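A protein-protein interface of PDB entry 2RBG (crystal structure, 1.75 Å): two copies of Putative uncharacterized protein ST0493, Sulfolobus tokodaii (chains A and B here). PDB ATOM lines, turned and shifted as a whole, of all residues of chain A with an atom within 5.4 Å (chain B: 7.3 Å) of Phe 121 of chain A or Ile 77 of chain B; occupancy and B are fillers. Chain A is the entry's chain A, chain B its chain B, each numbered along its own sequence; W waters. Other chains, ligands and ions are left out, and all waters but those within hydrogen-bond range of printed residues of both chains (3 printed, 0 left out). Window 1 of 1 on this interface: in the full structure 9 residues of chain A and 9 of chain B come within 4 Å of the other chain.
Ile 77 of chain B touches Asp 120 of chain A. Phe 121 of chain A touches Asp 76 of chain B. CG1 of Ile 77 of chain B touches CD1 of Phe 121 of chain A, 3.4 Å away. Lys 124 of chain A touches Trp 70 of chain B. O of Lys 124 of chain A touches CG2 of Ile 77 of chain B, 3.9 Å away. Lys 80 of chain B touches Leu 125 of chain A (CG to CD2, 3.9 Å). Leu 125 of chain A touches Asn 81 of chain B (CA to OD1, 3.5 Å).
No position is printed for both chains.
Water W1 bridges the side-chain carboxylate of Glu 74 of chain B (2.6 Å) and the backbone carbonyl oxygen of Asp 120 of chain A (2.8 Å). Water W2 bridges OE2 of Glu 74 of chain B (2.7 Å) and N of Asp 120 of chain A (2.8 Å). Water W3 bridges OE2 of Glu 74 of chain B and NZ of Lys 124 of chain A.
Of the printed residues of chain B, Phe 121 of chain A touches Asp 76 and Ile 77. Of the printed residues of chain A, Ile 77 of chain B touches Asp 120, Phe 121 and Lys 124. Of the printed residues of chain B, Lys 124 of chain A touches Trp 70, Glu 74, Ile 77 and Asn 81. Of the printed residues of chain B, Asp 120 of chain A touches Ile 77. Of the printed residues of chain A, Asp 76 of chain B touches Lys 23 (2.8 Å), Lys 119 (3.1 Å) and Phe 121 (3.4 Å). Printed residues of chain B within 4 Å of Lys 119 of chain A: Asn 73 and Asp 76. Tyr 93 of chain A touches none of the printed residues of chain B. Arg 123 of chain A touches none of the printed residues of chain B. The nearest printed residue of chain B that does not touch Leu 125 of chain A is Ile 77 of chain B (4.02 Å).
Of the 12 printed residues of chain A, 6 touch a printed residue of chain B. Hydrophobic or aromatic side chains of chain A that line the printed part of chain B: Phe 121 and Leu 125. Of the 12 printed residues of chain B, 7 touch a printed residue of chain A. Among the printed residues, Asp or Glu carboxylates within 4 Å of a Lys or Arg side-chain nitrogen of the other chain: Lys 23 of chain A with Asp 76 of chain B (2.8 Å), Lys 119 of chain A with Asp 76 of chain B (3.1 Å) and Lys 124 of chain A with Glu 74 of chain B (2.9 Å).
The side-chain carboxylate of Asp 76 of chain B lies within salt-bridge range of the side-chain amino group of Lys 23 of chain A, 2.8 Å away. The side-chain amino group (NZ) of Lys 119 of chain A is in hydrogen-bond range of the backbone carbonyl oxygen (O) of Asn 73 of chain B. NZ of Lys 119 of chain A lies within salt-bridge range of OD2 of Asp 76 of chain B, 3.1 Å away. The side-chain amino group of Lys 124 of chain A is in salt-bridge range of the side-chain carboxylate of Glu 74 of chain B, at 2.9 Å. The backbone carbonyl oxygen (O) of Lys 124 of chain A is in hydrogen-bond range of the side-chain amide nitrogen (ND2) of Asn 81 of chain B (3.0 Å).
O of Lys 119 of chain A lies within hydrogen-bond range of N of Val 92 of chain A, at 3.0 Å. N of Phe 121 of chain A lies within hydrogen-bond range of O of Val 92 of chain A, 2.8 Å away. OD2 of Asp 120 of chain A lies within salt-bridge range of NE of Arg 123 of chain A. The side-chain amide oxygen (OD1) of Asn 81 of chain B lies close to the backbone carbonyl oxygen (O) of Ile 77 of chain B (3.4 Å). The side-chain amino group of Lys 80 of chain B is in salt-bridge range of the side-chain carboxylate of Glu 83 of chain B (3.1 Å). The side-chain sulfur (SG) of Cys 122 of chain A forms a disulfide with the side-chain sulfur (SG) of Cys 94 of chain A (2.0 Å).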
ATOM      1  N   TYR A  20       1.682  12.204  11.570  1.00  0.00           N
ATOM      2  CA  TYR A  20       1.108  12.437  10.251  1.00  0.00           C
ATOM      3  C   TYR A  20       2.099  12.943   9.211  1.00  0.00           C
ATOM      4  O   TYR A  20       1.989  12.588   8.043  1.00  0.00           O
ATOM      5  CB  TYR A  20      -0.079  13.399  10.325  1.00  0.00           C
ATOM      6  CG  TYR A  20      -1.398  12.720  10.639  1.00  0.00           C
ATOM      7  CD1 TYR A  20      -1.639  12.166  11.896  1.00  0.00           C
ATOM      8  CD2 TYR A  20      -2.410  12.645   9.682  1.00  0.00           C
ATOM      9  CE1 TYR A  20      -2.859  11.560  12.193  1.00  0.00           C
ATOM     10  CE2 TYR A  20      -3.633  12.043   9.966  1.00  0.00           C
ATOM     11  CZ  TYR A  20      -3.850  11.504  11.230  1.00  0.00           C
ATOM     12  OH  TYR A  20      -5.068  10.935  11.535  1.00  0.00           O
ATOM     13  N   LYS A  23       3.745  10.253   7.501  1.00  0.00           N
ATOM     14  CA  LYS A  23       2.905   9.668   6.458  1.00  0.00           C
ATOM     15  C   LYS A  23       2.967  10.508   5.186  1.00  0.00           C
ATOM     16  O   LYS A  23       3.075   9.980   4.082  1.00  0.00           O
ATOM     17  CB  LYS A  23       1.445   9.584   6.914  1.00  0.00           C
ATOM     18  CG  LYS A  23       1.167   8.609   8.048  1.00  0.00           C
ATOM     19  CD  LYS A  23      -0.336   8.533   8.324  1.00  0.00           C
ATOM     20  CE  LYS A  23      -0.669   7.422   9.300  1.00  0.00           C
ATOM     21  NZ  LYS A  23      -0.298   6.086   8.751  1.00  0.00           N
ATOM     22  N   VAL A  92      -4.718  13.797   1.273  1.00  0.00           N
ATOM     23  CA  VAL A  92      -5.590  14.337   2.313  1.00  0.00           C
ATOM     24  C   VAL A  92      -5.406  13.625   3.651  1.00  0.00           C
ATOM     25  O   VAL A  92      -5.432  12.396   3.711  1.00  0.00           O
ATOM     26  CB  VAL A  92      -7.077  14.218   1.891  1.00  0.00           C
ATOM     27  CG1 VAL A  92      -7.983  14.671   3.024  1.00  0.00           C
ATOM     28  CG2 VAL A  92      -7.328  15.049   0.638  1.00  0.00           C
ATOM     29  N   TYR A  93      -5.238  14.404   4.717  1.00  0.00           N
ATOM     30  CA  TYR A  93      -5.054  13.845   6.058  1.00  0.00           C
ATOM     31  C   TYR A  93      -5.843  14.587   7.128  1.00  0.00           C
ATOM     32  O   TYR A  93      -5.912  15.816   7.126  1.00  0.00           O
ATOM     33  CB  TYR A  93      -3.582  13.899   6.466  1.00  0.00           C
ATOM     34  CG  TYR A  93      -2.638  13.286   5.469  1.00  0.00           C
ATOM     35  CD1 TYR A  93      -2.293  11.936   5.540  1.00  0.00           C
ATOM     36  CD2 TYR A  93      -2.097  14.055   4.442  1.00  0.00           C
ATOM     37  CE1 TYR A  93      -1.430  11.369   4.608  1.00  0.00           C
ATOM     38  CE2 TYR A  93      -1.241  13.503   3.511  1.00  0.00           C
ATOM     39  CZ  TYR A  93      -0.909  12.160   3.596  1.00  0.00           C
ATOM     40  OH  TYR A  93      -0.049  11.622   2.669  1.00  0.00           O
ATOM     41  N   CYS A  94      -6.416  13.830   8.058  1.00  0.00           N
ATOM     42  CA  CYS A  94      -7.160  14.418   9.165  1.00  0.00           C
ATOM     43  C   CYS A  94      -7.346  13.375  10.256  1.00  0.00           C
ATOM     44  O   CYS A  94      -7.075  12.189  10.044  1.00  0.00           O
ATOM     45  CB  CYS A  94      -8.545  14.901   8.705  1.00  0.00           C
ATOM     46  SG  CYS A  94      -9.828  13.603   8.594  1.00  0.00           S
ATOM     47  N   LYS A 119      -3.886   9.449  -1.847  1.00  0.00           N
ATOM     48  CA  LYS A 119      -4.096   8.813  -0.554  1.00  0.00           C
ATOM     49  C   LYS A 119      -4.960   9.724   0.295  1.00  0.00           C
ATOM     50  O   LYS A 119      -4.749  10.934   0.333  1.00  0.00           O
ATOM     51  CB  LYS A 119      -2.758   8.569   0.158  1.00  0.00           C
ATOM     52  CG  LYS A 119      -2.883   8.039   1.600  1.00  0.00           C
ATOM     53  CD  LYS A 119      -3.524   6.656   1.661  1.00  0.00           C
ATOM     54  CE  LYS A 119      -3.670   6.150   3.101  1.00  0.00           C
ATOM     55  NZ  LYS A 119      -2.359   5.806   3.726  1.00  0.00           N
ATOM     56  N   ASP A 120      -5.946   9.133   0.956  1.00  0.00           N
ATOM     57  CA  ASP A 120      -6.837   9.878   1.826  1.00  0.00           C
ATOM     58  C   ASP A 120      -6.857   9.166   3.173  1.00  0.00           C
ATOM     59  O   ASP A 120      -7.501   8.132   3.320  1.00  0.00           O
ATOM     60  CB  ASP A 120      -8.255   9.917   1.242  1.00  0.00           C
ATOM     61  CG  ASP A 120      -9.203  10.789   2.054  1.00  0.00           C
ATOM     62  OD1 ASP A 120      -9.276  10.613   3.289  1.00  0.00           O
ATOM     63  OD2 ASP A 120      -9.882  11.648   1.457  1.00  0.00           O
ATOM     64  N   PHE A 121      -6.104   9.686   4.135  1.00  0.00           N
ATOM     65  CA  PHE A 121      -6.107   9.104   5.470  1.00  0.00           C
ATOM     66  C   PHE A 121      -6.993  10.068   6.232  1.00  0.00           C
ATOM     67  O   PHE A 121      -6.511  10.916   6.986  1.00  0.00           O
ATOM     68  CB  PHE A 121      -4.707   9.094   6.083  1.00  0.00           C
ATOM     69  CG  PHE A 121      -4.614   8.280   7.343  1.00  0.00           C
ATOM     70  CD1 PHE A 121      -4.420   6.904   7.284  1.00  0.00           C
ATOM     71  CD2 PHE A 121      -4.760   8.882   8.586  1.00  0.00           C
ATOM     72  CE1 PHE A 121      -4.375   6.139   8.446  1.00  0.00           C
ATOM     73  CE2 PHE A 121      -4.719   8.124   9.757  1.00  0.00           C
ATOM     74  CZ  PHE A 121      -4.524   6.749   9.685  1.00  0.00           C
ATOM     75  N   CYS A 122      -8.299   9.948   6.018  1.00  0.00           N
ATOM     76  CA  CYS A 122      -9.233  10.853   6.659  1.00  0.00           C
ATOM     77  C   CYS A 122     -10.689  10.405   6.604  1.00  0.00           C
ATOM     78  O   CYS A 122     -11.250   9.962   7.606  1.00  0.00           O
ATOM     79  CB  CYS A 122      -9.091  12.236   6.013  1.00  0.00           C
ATOM     80  SG  CYS A 122     -10.267  13.486   6.614  1.00  0.00           S
ATOM     81  N   ARG A 123     -11.296  10.510   5.429  1.00  0.00           N
ATOM     82  CA  ARG A 123     -12.701  10.157   5.266  1.00  0.00           C
ATOM     83  C   ARG A 123     -13.123   8.728   5.610  1.00  0.00           C
ATOM     84  O   ARG A 123     -14.254   8.516   6.047  1.00  0.00           O
ATOM     85  CB  ARG A 123     -13.157  10.528   3.853  1.00  0.00           C
ATOM     86  CG  ARG A 123     -13.228  12.043   3.656  1.00  0.00           C
ATOM     87  CD  ARG A 123     -13.639  12.430   2.249  1.00  0.00           C
ATOM     88  NE  ARG A 123     -12.633  12.046   1.265  1.00  0.00           N
ATOM     89  CZ  ARG A 123     -12.752  12.245  -0.043  1.00  0.00           C
ATOM     90  NH1 ARG A 123     -13.838  12.829  -0.529  1.00  0.00           N
ATOM     91  NH2 ARG A 123     -11.786  11.859  -0.864  1.00  0.00           N
ATOM     92  N   LYS A 124     -12.235   7.753   5.433  1.00  0.00           N
ATOM     93  CA  LYS A 124     -12.588   6.372   5.761  1.00  0.00           C
ATOM     94  C   LYS A 124     -12.345   6.032   7.235  1.00  0.00           C
ATOM     95  O   LYS A 124     -12.612   4.911   7.664  1.00  0.00           O
ATOM     96  CB  LYS A 124     -11.818   5.379   4.875  1.00  0.00           C
ATOM     97  CG  LYS A 124     -12.339   5.253   3.438  1.00  0.00           C
ATOM     98  CD  LYS A 124     -11.562   4.185   2.666  1.00  0.00           C
ATOM     99  CE  LYS A 124     -12.091   3.991   1.247  1.00  0.00           C
ATOM    100  NZ  LYS A 124     -11.371   2.890   0.522  1.00  0.00           N
ATOM    101  N   LEU A 125     -11.836   6.987   8.009  1.00  0.00           N
ATOM    102  CA  LEU A 125     -11.590   6.743   9.429  1.00  0.00           C
ATOM    103  C   LEU A 125     -12.914   6.617  10.170  1.00  0.00           C
ATOM    104  O   LEU A 125     -13.837   7.395   9.939  1.00  0.00           O
ATOM    105  CB  LEU A 125     -10.780   7.884  10.046  1.00  0.00           C
ATOM    106  CG  LEU A 125      -9.305   7.988   9.671  1.00  0.00           C
ATOM    107  CD1 LEU A 125      -8.749   9.300  10.202  1.00  0.00           C
ATOM    108  CD2 LEU A 125      -8.535   6.804  10.249  1.00  0.00           C
ATOM    109  N   TRP B  70     -10.507  -1.787   0.776  1.00  0.00           N
ATOM    110  CA  TRP B  70      -9.290  -1.032   1.046  1.00  0.00           C
ATOM    111  C   TRP B  70      -8.262  -1.194  -0.057  1.00  0.00           C
ATOM    112  O   TRP B  70      -7.912  -2.318  -0.425  1.00  0.00           O
ATOM    113  CB  TRP B  70      -8.648  -1.494   2.360  1.00  0.00           C
ATOM    114  CG  TRP B  70      -9.578  -1.491   3.526  1.00  0.00           C
ATOM    115  CD1 TRP B  70     -10.154  -2.576   4.119  1.00  0.00           C
ATOM    116  CD2 TRP B  70     -10.039  -0.345   4.248  1.00  0.00           C
ATOM    117  NE1 TRP B  70     -10.948  -2.176   5.171  1.00  0.00           N
ATOM    118  CE2 TRP B  70     -10.893  -0.810   5.270  1.00  0.00           C
ATOM    119  CE3 TRP B  70      -9.812   1.033   4.128  1.00  0.00           C
ATOM    120  CZ2 TRP B  70     -11.523   0.055   6.173  1.00  0.00           C
ATOM    121  CZ3 TRP B  70     -10.438   1.893   5.022  1.00  0.00           C
ATOM    122  CH2 TRP B  70     -11.285   1.400   6.033  1.00  0.00           C
ATOM    123  N   ASN B  73      -2.695   0.914  -0.348  1.00  0.00           N
ATOM    124  CA  ASN B  73      -2.056   1.913   0.500  1.00  0.00           C
ATOM    125  C   ASN B  73      -2.953   2.379   1.647  1.00  0.00           C
ATOM    126  O   ASN B  73      -2.606   3.309   2.373  1.00  0.00           O
ATOM    127  CB  ASN B  73      -1.584   3.116  -0.346  1.00  0.00           C
ATOM    128  CG  ASN B  73      -2.730   3.903  -0.965  1.00  0.00           C
ATOM    129  OD1 ASN B  73      -3.852   3.413  -1.080  1.00  0.00           O
ATOM    130  ND2 ASN B  73      -2.439   5.132  -1.386  1.00  0.00           N
ATOM    131  N   GLU B  74      -4.090   1.710   1.830  1.00  0.00           N
ATOM    132  CA  GLU B  74      -5.017   2.087   2.892  1.00  0.00           C
ATOM    133  C   GLU B  74      -5.061   1.105   4.059  1.00  0.00           C
ATOM    134  O   GLU B  74      -5.959   1.173   4.897  1.00  0.00           O
ATOM    135  CB  GLU B  74      -6.427   2.257   2.323  1.00  0.00           C
ATOM    136  CG  GLU B  74      -6.516   3.293   1.207  1.00  0.00           C
ATOM    137  CD  GLU B  74      -7.914   3.416   0.642  1.00  0.00           C
ATOM    138  OE1 GLU B  74      -8.552   2.372   0.394  1.00  0.00           O
ATOM    139  OE2 GLU B  74      -8.372   4.559   0.433  1.00  0.00           O
ATOM    140  N   VAL B  75      -4.097   0.193   4.122  1.00  0.00           N
ATOM    141  CA  VAL B  75      -4.084  -0.767   5.214  1.00  0.00           C
ATOM    142  C   VAL B  75      -3.965  -0.045   6.555  1.00  0.00           C
ATOM    143  O   VAL B  75      -4.504  -0.504   7.559  1.00  0.00           O
ATOM    144  CB  VAL B  75      -2.928  -1.791   5.068  1.00  0.00           C
ATOM    145  CG1 VAL B  75      -2.878  -2.700   6.295  1.00  0.00           C
ATOM    146  CG2 VAL B  75      -3.139  -2.635   3.817  1.00  0.00           C
ATOM    147  N   ASP B  76      -3.275   1.092   6.579  1.00  0.00           N
ATOM    148  CA  ASP B  76      -3.136   1.812   7.837  1.00  0.00           C
ATOM    149  C   ASP B  76      -4.468   2.360   8.347  1.00  0.00           C
ATOM    150  O   ASP B  76      -4.666   2.470   9.555  1.00  0.00           O
ATOM    151  CB  ASP B  76      -2.079   2.928   7.729  1.00  0.00           C
ATOM    152  CG  ASP B  76      -2.379   3.945   6.640  1.00  0.00           C
ATOM    153  OD1 ASP B  76      -3.305   3.736   5.837  1.00  0.00           O
ATOM    154  OD2 ASP B  76      -1.659   4.964   6.589  1.00  0.00           O
ATOM    155  N   ILE B  77      -5.386   2.682   7.438  1.00  0.00           N
ATOM    156  CA  ILE B  77      -6.696   3.195   7.844  1.00  0.00           C
ATOM    157  C   ILE B  77      -7.471   2.042   8.481  1.00  0.00           C
ATOM    158  O   ILE B  77      -8.100   2.196   9.531  1.00  0.00           O
ATOM    159  CB  ILE B  77      -7.510   3.721   6.640  1.00  0.00           C
ATOM    160  CG1 ILE B  77      -6.733   4.816   5.912  1.00  0.00           C
ATOM    161  CG2 ILE B  77      -8.843   4.289   7.124  1.00  0.00           C
ATOM    162  CD1 ILE B  77      -7.416   5.299   4.640  1.00  0.00           C
ATOM    163  N   PHE B  78      -7.419   0.888   7.823  1.00  0.00           N
ATOM    164  CA  PHE B  78      -8.080  -0.321   8.306  1.00  0.00           C
ATOM    165  C   PHE B  78      -7.584  -0.668   9.714  1.00  0.00           C
ATOM    166  O   PHE B  78      -8.376  -0.912  10.629  1.00  0.00           O
ATOM    167  CB  PHE B  78      -7.777  -1.478   7.345  1.00  0.00           C
ATOM    168  CG  PHE B  78      -7.951  -2.837   7.957  1.00  0.00           C
ATOM    169  CD1 PHE B  78      -9.220  -3.330   8.248  1.00  0.00           C
ATOM    170  CD2 PHE B  78      -6.841  -3.613   8.273  1.00  0.00           C
ATOM    171  CE1 PHE B  78      -9.382  -4.577   8.848  1.00  0.00           C
ATOM    172  CE2 PHE B  78      -6.992  -4.860   8.875  1.00  0.00           C
ATOM    173  CZ  PHE B  78      -8.267  -5.342   9.163  1.00  0.00           C
ATOM    174  N   LEU B  79      -6.267  -0.691   9.886  1.00  0.00           N
ATOM    175  CA  LEU B  79      -5.686  -1.019  11.184  1.00  0.00           C
ATOM    176  C   LEU B  79      -6.054  -0.011  12.270  1.00  0.00           C
ATOM    177  O   LEU B  79      -6.292  -0.386  13.420  1.00  0.00           O
ATOM    178  CB  LEU B  79      -4.162  -1.134  11.069  1.00  0.00           C
ATOM    179  CG  LEU B  79      -3.626  -2.343  10.290  1.00  0.00           C
ATOM    180  CD1 LEU B  79      -2.104  -2.301  10.260  1.00  0.00           C
ATOM    181  CD2 LEU B  79      -4.101  -3.635  10.945  1.00  0.00           C
ATOM    182  N   LYS B  80      -6.101   1.267  11.907  1.00  0.00           N
ATOM    183  CA  LYS B  80      -6.452   2.310  12.869  1.00  0.00           C
ATOM    184  C   LYS B  80      -7.888   2.125  13.351  1.00  0.00           C
ATOM    185  O   LYS B  80      -8.176   2.242  14.546  1.00  0.00           O
ATOM    186  CB  LYS B  80      -6.301   3.695  12.232  1.00  0.00           C
ATOM    187  CG  LYS B  80      -6.699   4.855  13.144  1.00  0.00           C
ATOM    188  CD  LYS B  80      -5.802   4.940  14.373  1.00  0.00           C
ATOM    189  CE  LYS B  80      -6.169   6.133  15.244  1.00  0.00           C
ATOM    190  NZ  LYS B  80      -7.575   6.052  15.721  1.00  0.00           N
ATOM    191  N   ASN B  81      -8.784   1.829  12.418  1.00  0.00           N
ATOM    192  CA  ASN B  81     -10.190   1.632  12.741  1.00  0.00           C
ATOM    193  C   ASN B  81     -10.419   0.428  13.648  1.00  0.00           C
ATOM    194  O   ASN B  81     -11.414   0.374  14.367  1.00  0.00           O
ATOM    195  CB  ASN B  81     -11.013   1.463  11.463  1.00  0.00           C
ATOM    196  CG  ASN B  81     -11.144   2.750  10.676  1.00  0.00           C
ATOM    197  OD1 ASN B  81     -10.618   3.795  11.066  1.00  0.00           O
ATOM    198  ND2 ASN B  81     -11.854   2.680   9.556  1.00  0.00           N
ATOM    199  N   LEU B  82      -9.506  -0.538  13.616  1.00  0.00           N
ATOM    200  CA  LEU B  82      -9.656  -1.718  14.460  1.00  0.00           C
ATOM    201  C   LEU B  82      -9.584  -1.368  15.940  1.00  0.00           C
ATOM    202  O   LEU B  82     -10.035  -2.134  16.789  1.00  0.00           O
ATOM    203  CB  LEU B  82      -8.582  -2.759  14.135  1.00  0.00           C
ATOM    204  CG  LEU B  82      -8.742  -3.522  12.821  1.00  0.00           C
ATOM    205  CD1 LEU B  82      -7.614  -4.541  12.695  1.00  0.00           C
ATOM    206  CD2 LEU B  82     -10.092  -4.225  12.789  1.00  0.00           C
ATOM    207  N   GLU B  83      -9.019  -0.209  16.255  1.00  0.00           N
ATOM    208  CA  GLU B  83      -8.919   0.200  17.649  1.00  0.00           C
ATOM    209  C   GLU B  83     -10.311   0.372  18.253  1.00  0.00           C
ATOM    210  O   GLU B  83     -10.484   0.270  19.468  1.00  0.00           O
ATOM    211  CB  GLU B  83      -8.136   1.508  17.766  1.00  0.00           C
ATOM    212  CG  GLU B  83      -6.779   1.469  17.084  1.00  0.00           C
ATOM    213  CD  GLU B  83      -5.910   2.660  17.436  1.00  0.00           C
ATOM    214  OE1 GLU B  83      -6.446   3.784  17.518  1.00  0.00           O
ATOM    215  OE2 GLU B  83      -4.689   2.469  17.619  1.00  0.00           O
HETATM  216  O   HOH W   1      -9.214   6.612   1.774  1.00  0.00           O
HETATM  217  O   HOH W   2      -6.828   6.714  -0.051  1.00  0.00           O
HETATM  218  O   HOH W   3     -10.177   4.755  -1.590  1.00  0.00           O
